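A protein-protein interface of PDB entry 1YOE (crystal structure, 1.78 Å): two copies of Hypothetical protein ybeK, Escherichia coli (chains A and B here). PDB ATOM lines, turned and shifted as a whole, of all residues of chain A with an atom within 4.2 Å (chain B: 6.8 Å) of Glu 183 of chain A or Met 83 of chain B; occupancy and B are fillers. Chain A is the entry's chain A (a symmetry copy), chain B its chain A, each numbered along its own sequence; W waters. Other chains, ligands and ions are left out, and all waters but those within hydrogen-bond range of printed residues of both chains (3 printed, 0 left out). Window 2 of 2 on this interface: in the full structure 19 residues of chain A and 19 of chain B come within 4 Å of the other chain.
The side-chain amide nitrogen (NE2) of Gln 277 of chain B lies within hydrogen-bond range of the backbone carbonyl oxygen (O) of Thr 276 of chain A, at 3.2 Å.
The backbone carbonyl oxygen (O) of Met 83 of chain B lies within hydrogen-bond range of the side-chain amide nitrogen (NE2) of Gln 190 of chain A (3.5 Å).
OE1 of Glu 183 of chain B is in salt-bridge range of NE of Arg 84 of chain B (2.8 Å).
The side-chain carboxylate (OE1) of Glu 183 of chain A lies within salt-bridge range of the guanidinium group (NE) of Arg 84 of chain A (2.8 Å).
The side-chain amide nitrogen (NE2) of Gln 190 of chain A is in hydrogen-bond range of the side-chain carboxylate (OE2) of Glu 186 of chain A (3.0 Å).
NH2 of Arg 84 of chain A lies within hydrogen-bond range of O of Thr 276 of chain A (3.2 Å).
The side-chain carboxylate of Asp 181 of chain B lies within hydrogen-bond range of the backbone NH of Leu 82 of chain B.
Among the printed residues, merely in contact across the chains: Ile 187 of chain A with Leu 82 of chain B (3.5 Å), Ile 187 of chain A with Met 83 of chain B (3.7 Å), Met 83 of chain A with Glu 183 of chain B (3.7 Å), Glu 183 of chain A with Met 83 of chain B (3.7 Å) and Glu 186 of chain A with Met 83 of chain B (3.8 Å).
Printed residues of chain B within 4 Å of Met 83 of chain A: Glu 183.
Glu 183 of chain A touches one residue of chain B.
Ala 184 of chain A touches none of the printed residues of chain B.
Of the printed residues of chain B, Glu 186 of chain A touches Met 83 (3.8 Å).
Of the printed residues of chain A, Gln 277 of chain B touches Thr 276.
The nearest printed residue of chain A that does not touch Met 83 of chain B is Thr 276 of chain A (4.3 Å).
Of the 11 printed residues of chain A, 6 touch a printed residue of chain B.
Of the 10 printed residues of chain B, 4 touch a printed residue of chain A.
Hydrophobic or aromatic side chains of chain B within 4 Å of the printed part of chain A: Met 83.
Among the printed residues, no Asp or Glu carboxylate lies within 4 Å of a Lys or Arg side-chain nitrogen of the other chain.
Met 83 of chain A touches Glu 183 of chain B, and with the chains exchanged Glu 183 of chain A touches Met 83 of chain B.
5 positions are printed for both chains.
Of the 7 pairs that touch across the chains among the printed residues, 2 have their exchanged pair printed and touching as well.
Water W1 lies within hydrogen-bond range of OE1 of Gln 190 of chain A (2.8 Å), O of Leu 82 of chain B (2.9 Å) and NZ of Lys 80 of chain B (3.2 Å).
Water W3 lies within hydrogen-bond range of NZ of Lys 80 of chain B (2.8 Å), OE2 of Glu 85 of chain B (3.2 Å) and OE1 of Gln 190 of chain A (3.3 Å).
Water W2 lies within hydrogen-bond range of O of Gln 190 of chain A (3.1 Å) and NZ of Lys 80 of chain B (3.5 Å).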
ATOM      1  N   MET A  83     -10.431  15.877  -0.681  1.00  0.00           N
ATOM      2  CA  MET A  83     -11.123  15.098   0.338  1.00  0.00           C
ATOM      3  C   MET A  83     -12.435  15.707   0.801  1.00  0.00           C
ATOM      4  O   MET A  83     -12.990  15.294   1.832  1.00  0.00           O
ATOM      5  CB  MET A  83     -10.222  14.968   1.552  1.00  0.00           C
ATOM      6  CG  MET A  83      -8.966  14.218   1.282  1.00  0.00           C
ATOM      7  SD  MET A  83      -8.140  13.987   2.813  1.00  0.00           S
ATOM      8  CE  MET A  83      -9.116  12.794   3.532  1.00  0.00           C
ATOM      9  N   ARG A  84     -12.911  16.697   0.053  1.00  0.00           N
ATOM     10  CA  ARG A  84     -14.092  17.461   0.434  1.00  0.00           C
ATOM     11  C   ARG A  84     -14.959  17.692  -0.777  1.00  0.00           C
ATOM     12  O   ARG A  84     -14.483  17.635  -1.916  1.00  0.00           O
ATOM     13  CB  ARG A  84     -13.677  18.820   1.007  1.00  0.00           C
ATOM     14  CG  ARG A  84     -12.850  18.708   2.253  1.00  0.00           C
ATOM     15  CD  ARG A  84     -12.375  20.023   2.838  1.00  0.00           C
ATOM     16  NE  ARG A  84     -11.436  19.700   3.906  1.00  0.00           N
ATOM     17  CZ  ARG A  84     -11.550  20.068   5.174  1.00  0.00           C
ATOM     18  NH1 ARG A  84     -12.578  20.818   5.578  1.00  0.00           N
ATOM     19  NH2 ARG A  84     -10.622  19.677   6.044  1.00  0.00           N
ATOM     20  N   ASP A 181     -10.080  23.795  -0.175  1.00  0.00           N
ATOM     21  CA  ASP A 181      -9.264  22.590  -0.157  1.00  0.00           C
ATOM     22  C   ASP A 181      -8.070  22.742   0.800  1.00  0.00           C
ATOM     23  O   ASP A 181      -6.952  23.027   0.377  1.00  0.00           O
ATOM     24  CB  ASP A 181      -8.834  22.215  -1.584  1.00  0.00           C
ATOM     25  CG  ASP A 181      -8.375  20.775  -1.693  1.00  0.00           C
ATOM     26  OD1 ASP A 181      -8.019  20.157  -0.666  1.00  0.00           O
ATOM     27  OD2 ASP A 181      -8.311  20.199  -2.799  1.00  0.00           O
ATOM     28  N   PRO A 182      -8.315  22.565   2.102  1.00  0.00           N
ATOM     29  CA  PRO A 182      -7.258  22.754   3.103  1.00  0.00           C
ATOM     30  C   PRO A 182      -6.154  21.720   2.961  1.00  0.00           C
ATOM     31  O   PRO A 182      -4.987  22.086   3.089  1.00  0.00           O
ATOM     32  CB  PRO A 182      -7.996  22.618   4.439  1.00  0.00           C
ATOM     33  CG  PRO A 182      -9.431  22.877   4.114  1.00  0.00           C
ATOM     34  CD  PRO A 182      -9.614  22.263   2.728  1.00  0.00           C
ATOM     35  N   GLU A 183      -6.528  20.469   2.687  1.00  0.00           N
ATOM     36  CA  GLU A 183      -5.548  19.399   2.498  1.00  0.00           C
ATOM     37  C   GLU A 183      -4.581  19.706   1.344  1.00  0.00           C
ATOM     38  O   GLU A 183      -3.357  19.537   1.483  1.00  0.00           O
ATOM     39  CB  GLU A 183      -6.270  18.073   2.263  1.00  0.00           C
ATOM     40  CG  GLU A 183      -6.940  17.505   3.518  1.00  0.00           C
ATOM     41  CD  GLU A 183      -8.310  18.093   3.855  1.00  0.00           C
ATOM     42  OE1 GLU A 183      -8.953  18.762   3.026  1.00  0.00           O
ATOM     43  OE2 GLU A 183      -8.770  17.858   4.992  1.00  0.00           O
ATOM     44  N   ALA A 184      -5.111  20.181   0.221  1.00  0.00           N
ATOM     45  CA  ALA A 184      -4.240  20.558  -0.910  1.00  0.00           C
ATOM     46  C   ALA A 184      -3.283  21.688  -0.555  1.00  0.00           C
ATOM     47  O   ALA A 184      -2.096  21.664  -0.929  1.00  0.00           O
ATOM     48  CB  ALA A 184      -5.044  20.933  -2.125  1.00  0.00           C
ATOM     49  N   ALA A 185      -3.795  22.683   0.159  1.00  0.00           N
ATOM     50  CA  ALA A 185      -2.941  23.798   0.589  1.00  0.00           C
ATOM     51  C   ALA A 185      -1.847  23.308   1.523  1.00  0.00           C
ATOM     52  O   ALA A 185      -0.688  23.706   1.373  1.00  0.00           O
ATOM     53  CB  ALA A 185      -3.761  24.887   1.252  1.00  0.00           C
ATOM     54  N   GLU A 186      -2.209  22.439   2.471  1.00  0.00           N
ATOM     55  CA  GLU A 186      -1.222  21.871   3.403  1.00  0.00           C
ATOM     56  C   GLU A 186      -0.140  21.101   2.634  1.00  0.00           C
ATOM     57  O   GLU A 186       1.045  21.225   2.950  1.00  0.00           O
ATOM     58  CB  GLU A 186      -1.891  21.002   4.490  1.00  0.00           C
ATOM     59  CG  GLU A 186      -0.935  20.267   5.452  1.00  0.00           C
ATOM     60  CD  GLU A 186      -0.130  21.152   6.399  1.00  0.00           C
ATOM     61  OE1 GLU A 186      -0.055  22.389   6.236  1.00  0.00           O
ATOM     62  OE2 GLU A 186       0.468  20.577   7.342  1.00  0.00           O
ATOM     63  N   ILE A 187      -0.541  20.337   1.615  1.00  0.00           N
ATOM     64  CA  ILE A 187       0.432  19.613   0.783  1.00  0.00           C
ATOM     65  C   ILE A 187       1.434  20.585   0.134  1.00  0.00           C
ATOM     66  O   ILE A 187       2.648  20.338   0.133  1.00  0.00           O
ATOM     67  CB  ILE A 187      -0.284  18.735  -0.263  1.00  0.00           C
ATOM     68  CG1 ILE A 187      -0.943  17.527   0.429  1.00  0.00           C
ATOM     69  CG2 ILE A 187       0.686  18.283  -1.399  1.00  0.00           C
ATOM     70  CD1 ILE A 187      -2.082  16.849  -0.374  1.00  0.00           C
ATOM     71  N   GLN A 190       3.851  21.961   2.835  1.00  0.00           N
ATOM     72  CA  GLN A 190       4.736  20.877   3.319  1.00  0.00           C
ATOM     73  C   GLN A 190       5.712  20.349   2.253  1.00  0.00           C
ATOM     74  O   GLN A 190       6.512  19.448   2.536  1.00  0.00           O
ATOM     75  CB  GLN A 190       3.915  19.635   3.713  1.00  0.00           C
ATOM     76  CG  GLN A 190       3.095  19.645   4.994  1.00  0.00           C
ATOM     77  CD  GLN A 190       2.313  18.318   5.173  1.00  0.00           C
ATOM     78  OE1 GLN A 190       2.148  17.536   4.216  1.00  0.00           O
ATOM     79  NE2 GLN A 190       1.847  18.064   6.391  1.00  0.00           N
ATOM     80  N   THR A 276      -6.201  21.461   9.117  1.00  0.00           N
ATOM     81  CA  THR A 276      -7.131  20.579   8.396  1.00  0.00           C
ATOM     82  C   THR A 276      -8.085  19.795   9.301  1.00  0.00           C
ATOM     83  O   THR A 276      -9.004  19.137   8.797  1.00  0.00           O
ATOM     84  CB  THR A 276      -6.371  19.582   7.487  1.00  0.00           C
ATOM     85  OG1 THR A 276      -5.456  18.819   8.282  1.00  0.00           O
ATOM     86  CG2 THR A 276      -5.470  20.329   6.491  1.00  0.00           C
ATOM     87  N   LYS B  80       6.057   8.871  -1.049  1.00  0.00           N
ATOM     88  CA  LYS B  80       5.584   9.046   0.326  1.00  0.00           C
ATOM     89  C   LYS B  80       4.061   9.227   0.351  1.00  0.00           C
ATOM     90  O   LYS B  80       3.452   9.476  -0.702  1.00  0.00           O
ATOM     91  CB  LYS B  80       6.283  10.261   0.968  1.00  0.00           C
ATOM     92  CG  LYS B  80       5.922  11.581   0.316  1.00  0.00           C
ATOM     93  CD  LYS B  80       6.638  12.765   0.980  1.00  0.00           C
ATOM     94  CE  LYS B  80       5.980  13.182   2.289  1.00  0.00           C
ATOM     95  NZ  LYS B  80       4.553  13.621   2.115  1.00  0.00           N
ATOM     96  N   PRO B  81       3.448   9.110   1.534  1.00  0.00           N
ATOM     97  CA  PRO B  81       2.015   9.402   1.700  1.00  0.00           C
ATOM     98  C   PRO B  81       1.639  10.812   1.282  1.00  0.00           C
ATOM     99  O   PRO B  81       2.499  11.704   1.232  1.00  0.00           O
ATOM    100  CB  PRO B  81       1.799   9.240   3.210  1.00  0.00           C
ATOM    101  CG  PRO B  81       2.823   8.225   3.601  1.00  0.00           C
ATOM    102  CD  PRO B  81       4.047   8.626   2.795  1.00  0.00           C
ATOM    103  N   LEU B  82       0.355  11.005   0.984  1.00  0.00           N
ATOM    104  CA  LEU B  82      -0.133  12.307   0.531  1.00  0.00           C
ATOM    105  C   LEU B  82       0.247  13.474   1.439  1.00  0.00           C
ATOM    106  O   LEU B  82       0.730  14.507   0.963  1.00  0.00           O
ATOM    107  CB  LEU B  82      -1.658  12.270   0.374  1.00  0.00           C
ATOM    108  CG  LEU B  82      -2.191  11.231  -0.614  1.00  0.00           C
ATOM    109  CD1 LEU B  82      -3.710  11.341  -0.673  1.00  0.00           C
ATOM    110  CD2 LEU B  82      -1.577  11.413  -2.017  1.00  0.00           C
ATOM    111  N   MET B  83       0.007  13.297   2.737  1.00  0.00           N
ATOM    112  CA  MET B  83       0.121  14.375   3.710  1.00  0.00           C
ATOM    113  C   MET B  83       0.942  14.020   4.937  1.00  0.00           C
ATOM    114  O   MET B  83       0.905  14.741   5.948  1.00  0.00           O
ATOM    115  CB  MET B  83      -1.269  14.759   4.181  1.00  0.00           C
ATOM    116  CG  MET B  83      -2.133  15.305   3.101  1.00  0.00           C
ATOM    117  SD  MET B  83      -3.618  15.878   3.840  1.00  0.00           S
ATOM    118  CE  MET B  83      -3.073  17.295   4.608  1.00  0.00           C
ATOM    119  N   ARG B  84       1.660  12.905   4.853  1.00  0.00           N
ATOM    120  CA  ARG B  84       2.402  12.370   5.987  1.00  0.00           C
ATOM    121  C   ARG B  84       3.753  11.887   5.527  1.00  0.00           C
ATOM    122  O   ARG B  84       3.951  11.594   4.343  1.00  0.00           O
ATOM    123  CB  ARG B  84       1.642  11.189   6.602  1.00  0.00           C
ATOM    124  CG  ARG B  84       0.296  11.570   7.143  1.00  0.00           C
ATOM    125  CD  ARG B  84      -0.517  10.431   7.723  1.00  0.00           C
ATOM    126  NE  ARG B  84      -1.848  10.957   8.005  1.00  0.00           N
ATOM    127  CZ  ARG B  84      -2.445  10.958   9.187  1.00  0.00           C
ATOM    128  NH1 ARG B  84      -1.844  10.430  10.257  1.00  0.00           N
ATOM    129  NH2 ARG B  84      -3.657  11.496   9.296  1.00  0.00           N
ATOM    130  N   GLU B  85       4.690  11.805   6.468  1.00  0.00           N
ATOM    131  CA  GLU B  85       5.996  11.252   6.156  1.00  0.00           C
ATOM    132  C   GLU B  85       5.845   9.749   6.063  1.00  0.00           C
ATOM    133  O   GLU B  85       4.951   9.159   6.680  1.00  0.00           O
ATOM    134  CB  GLU B  85       7.030  11.626   7.233  1.00  0.00           C
ATOM    135  CG  GLU B  85       7.400  13.104   7.286  1.00  0.00           C
ATOM    136  CD  GLU B  85       7.846  13.669   5.948  1.00  0.00           C
ATOM    137  OE1 GLU B  85       8.675  13.034   5.259  1.00  0.00           O
ATOM    138  OE2 GLU B  85       7.366  14.768   5.590  1.00  0.00           O
ATOM    139  N   ASP B 181      -1.181   5.813   5.115  1.00  0.00           N
ATOM    140  CA  ASP B 181      -1.786   6.909   4.373  1.00  0.00           C
ATOM    141  C   ASP B 181      -3.313   6.929   4.560  1.00  0.00           C
ATOM    142  O   ASP B 181      -4.061   6.452   3.711  1.00  0.00           O
ATOM    143  CB  ASP B 181      -1.373   6.847   2.895  1.00  0.00           C
ATOM    144  CG  ASP B 181      -1.592   8.162   2.174  1.00  0.00           C
ATOM    145  OD1 ASP B 181      -2.384   9.005   2.648  1.00  0.00           O
ATOM    146  OD2 ASP B 181      -1.021   8.408   1.091  1.00  0.00           O
ATOM    147  N   GLU B 183      -5.431   9.500   4.656  1.00  0.00           N
ATOM    148  CA  GLU B 183      -6.077  10.398   3.699  1.00  0.00           C
ATOM    149  C   GLU B 183      -6.317   9.713   2.345  1.00  0.00           C
ATOM    150  O   GLU B 183      -7.414   9.817   1.769  1.00  0.00           O
ATOM    151  CB  GLU B 183      -5.238  11.663   3.528  1.00  0.00           C
ATOM    152  CG  GLU B 183      -5.283  12.602   4.737  1.00  0.00           C
ATOM    153  CD  GLU B 183      -4.344  12.237   5.887  1.00  0.00           C
ATOM    154  OE1 GLU B 183      -3.417  11.421   5.737  1.00  0.00           O
ATOM    155  OE2 GLU B 183      -4.532  12.808   6.982  1.00  0.00           O
ATOM    156  N   THR B 276      -9.157  10.272   9.944  1.00  0.00           N
ATOM    157  CA  THR B 276      -7.921  10.995   9.609  1.00  0.00           C
ATOM    158  C   THR B 276      -7.525  12.068  10.626  1.00  0.00           C
ATOM    159  O   THR B 276      -6.430  12.635  10.522  1.00  0.00           O
ATOM    160  CB  THR B 276      -8.010  11.645   8.206  1.00  0.00           C
ATOM    161  OG1 THR B 276      -9.143  12.520   8.161  1.00  0.00           O
ATOM    162  CG2 THR B 276      -8.311  10.586   7.133  1.00  0.00           C
ATOM    163  N   GLN B 277      -8.382  12.309  11.621  1.00  0.00           N
ATOM    164  CA  GLN B 277      -8.206  13.441  12.544  1.00  0.00           C
ATOM    165  C   GLN B 277      -8.038  13.063  14.023  1.00  0.00           C
ATOM    166  O   GLN B 277      -7.493  13.853  14.808  1.00  0.00           O
ATOM    167  CB  GLN B 277      -9.377  14.415  12.382  1.00  0.00           C
ATOM    168  CG  GLN B 277      -9.574  14.915  10.947  1.00  0.00           C
ATOM    169  CD  GLN B 277     -10.719  15.905  10.802  1.00  0.00           C
ATOM    170  OE1 GLN B 277     -11.562  16.032  11.694  1.00  0.00           O
ATOM    171  NE2 GLN B 277     -10.753  16.606   9.669  1.00  0.00           N
HETATM  172  O   HOH W   1       2.797  16.325   1.809  1.00  0.00           O
HETATM  173  O   HOH W   2       6.494  16.480   1.657  1.00  0.00           O
HETATM  174  O   HOH W   3       4.359  15.111   4.491  1.00  0.00           O
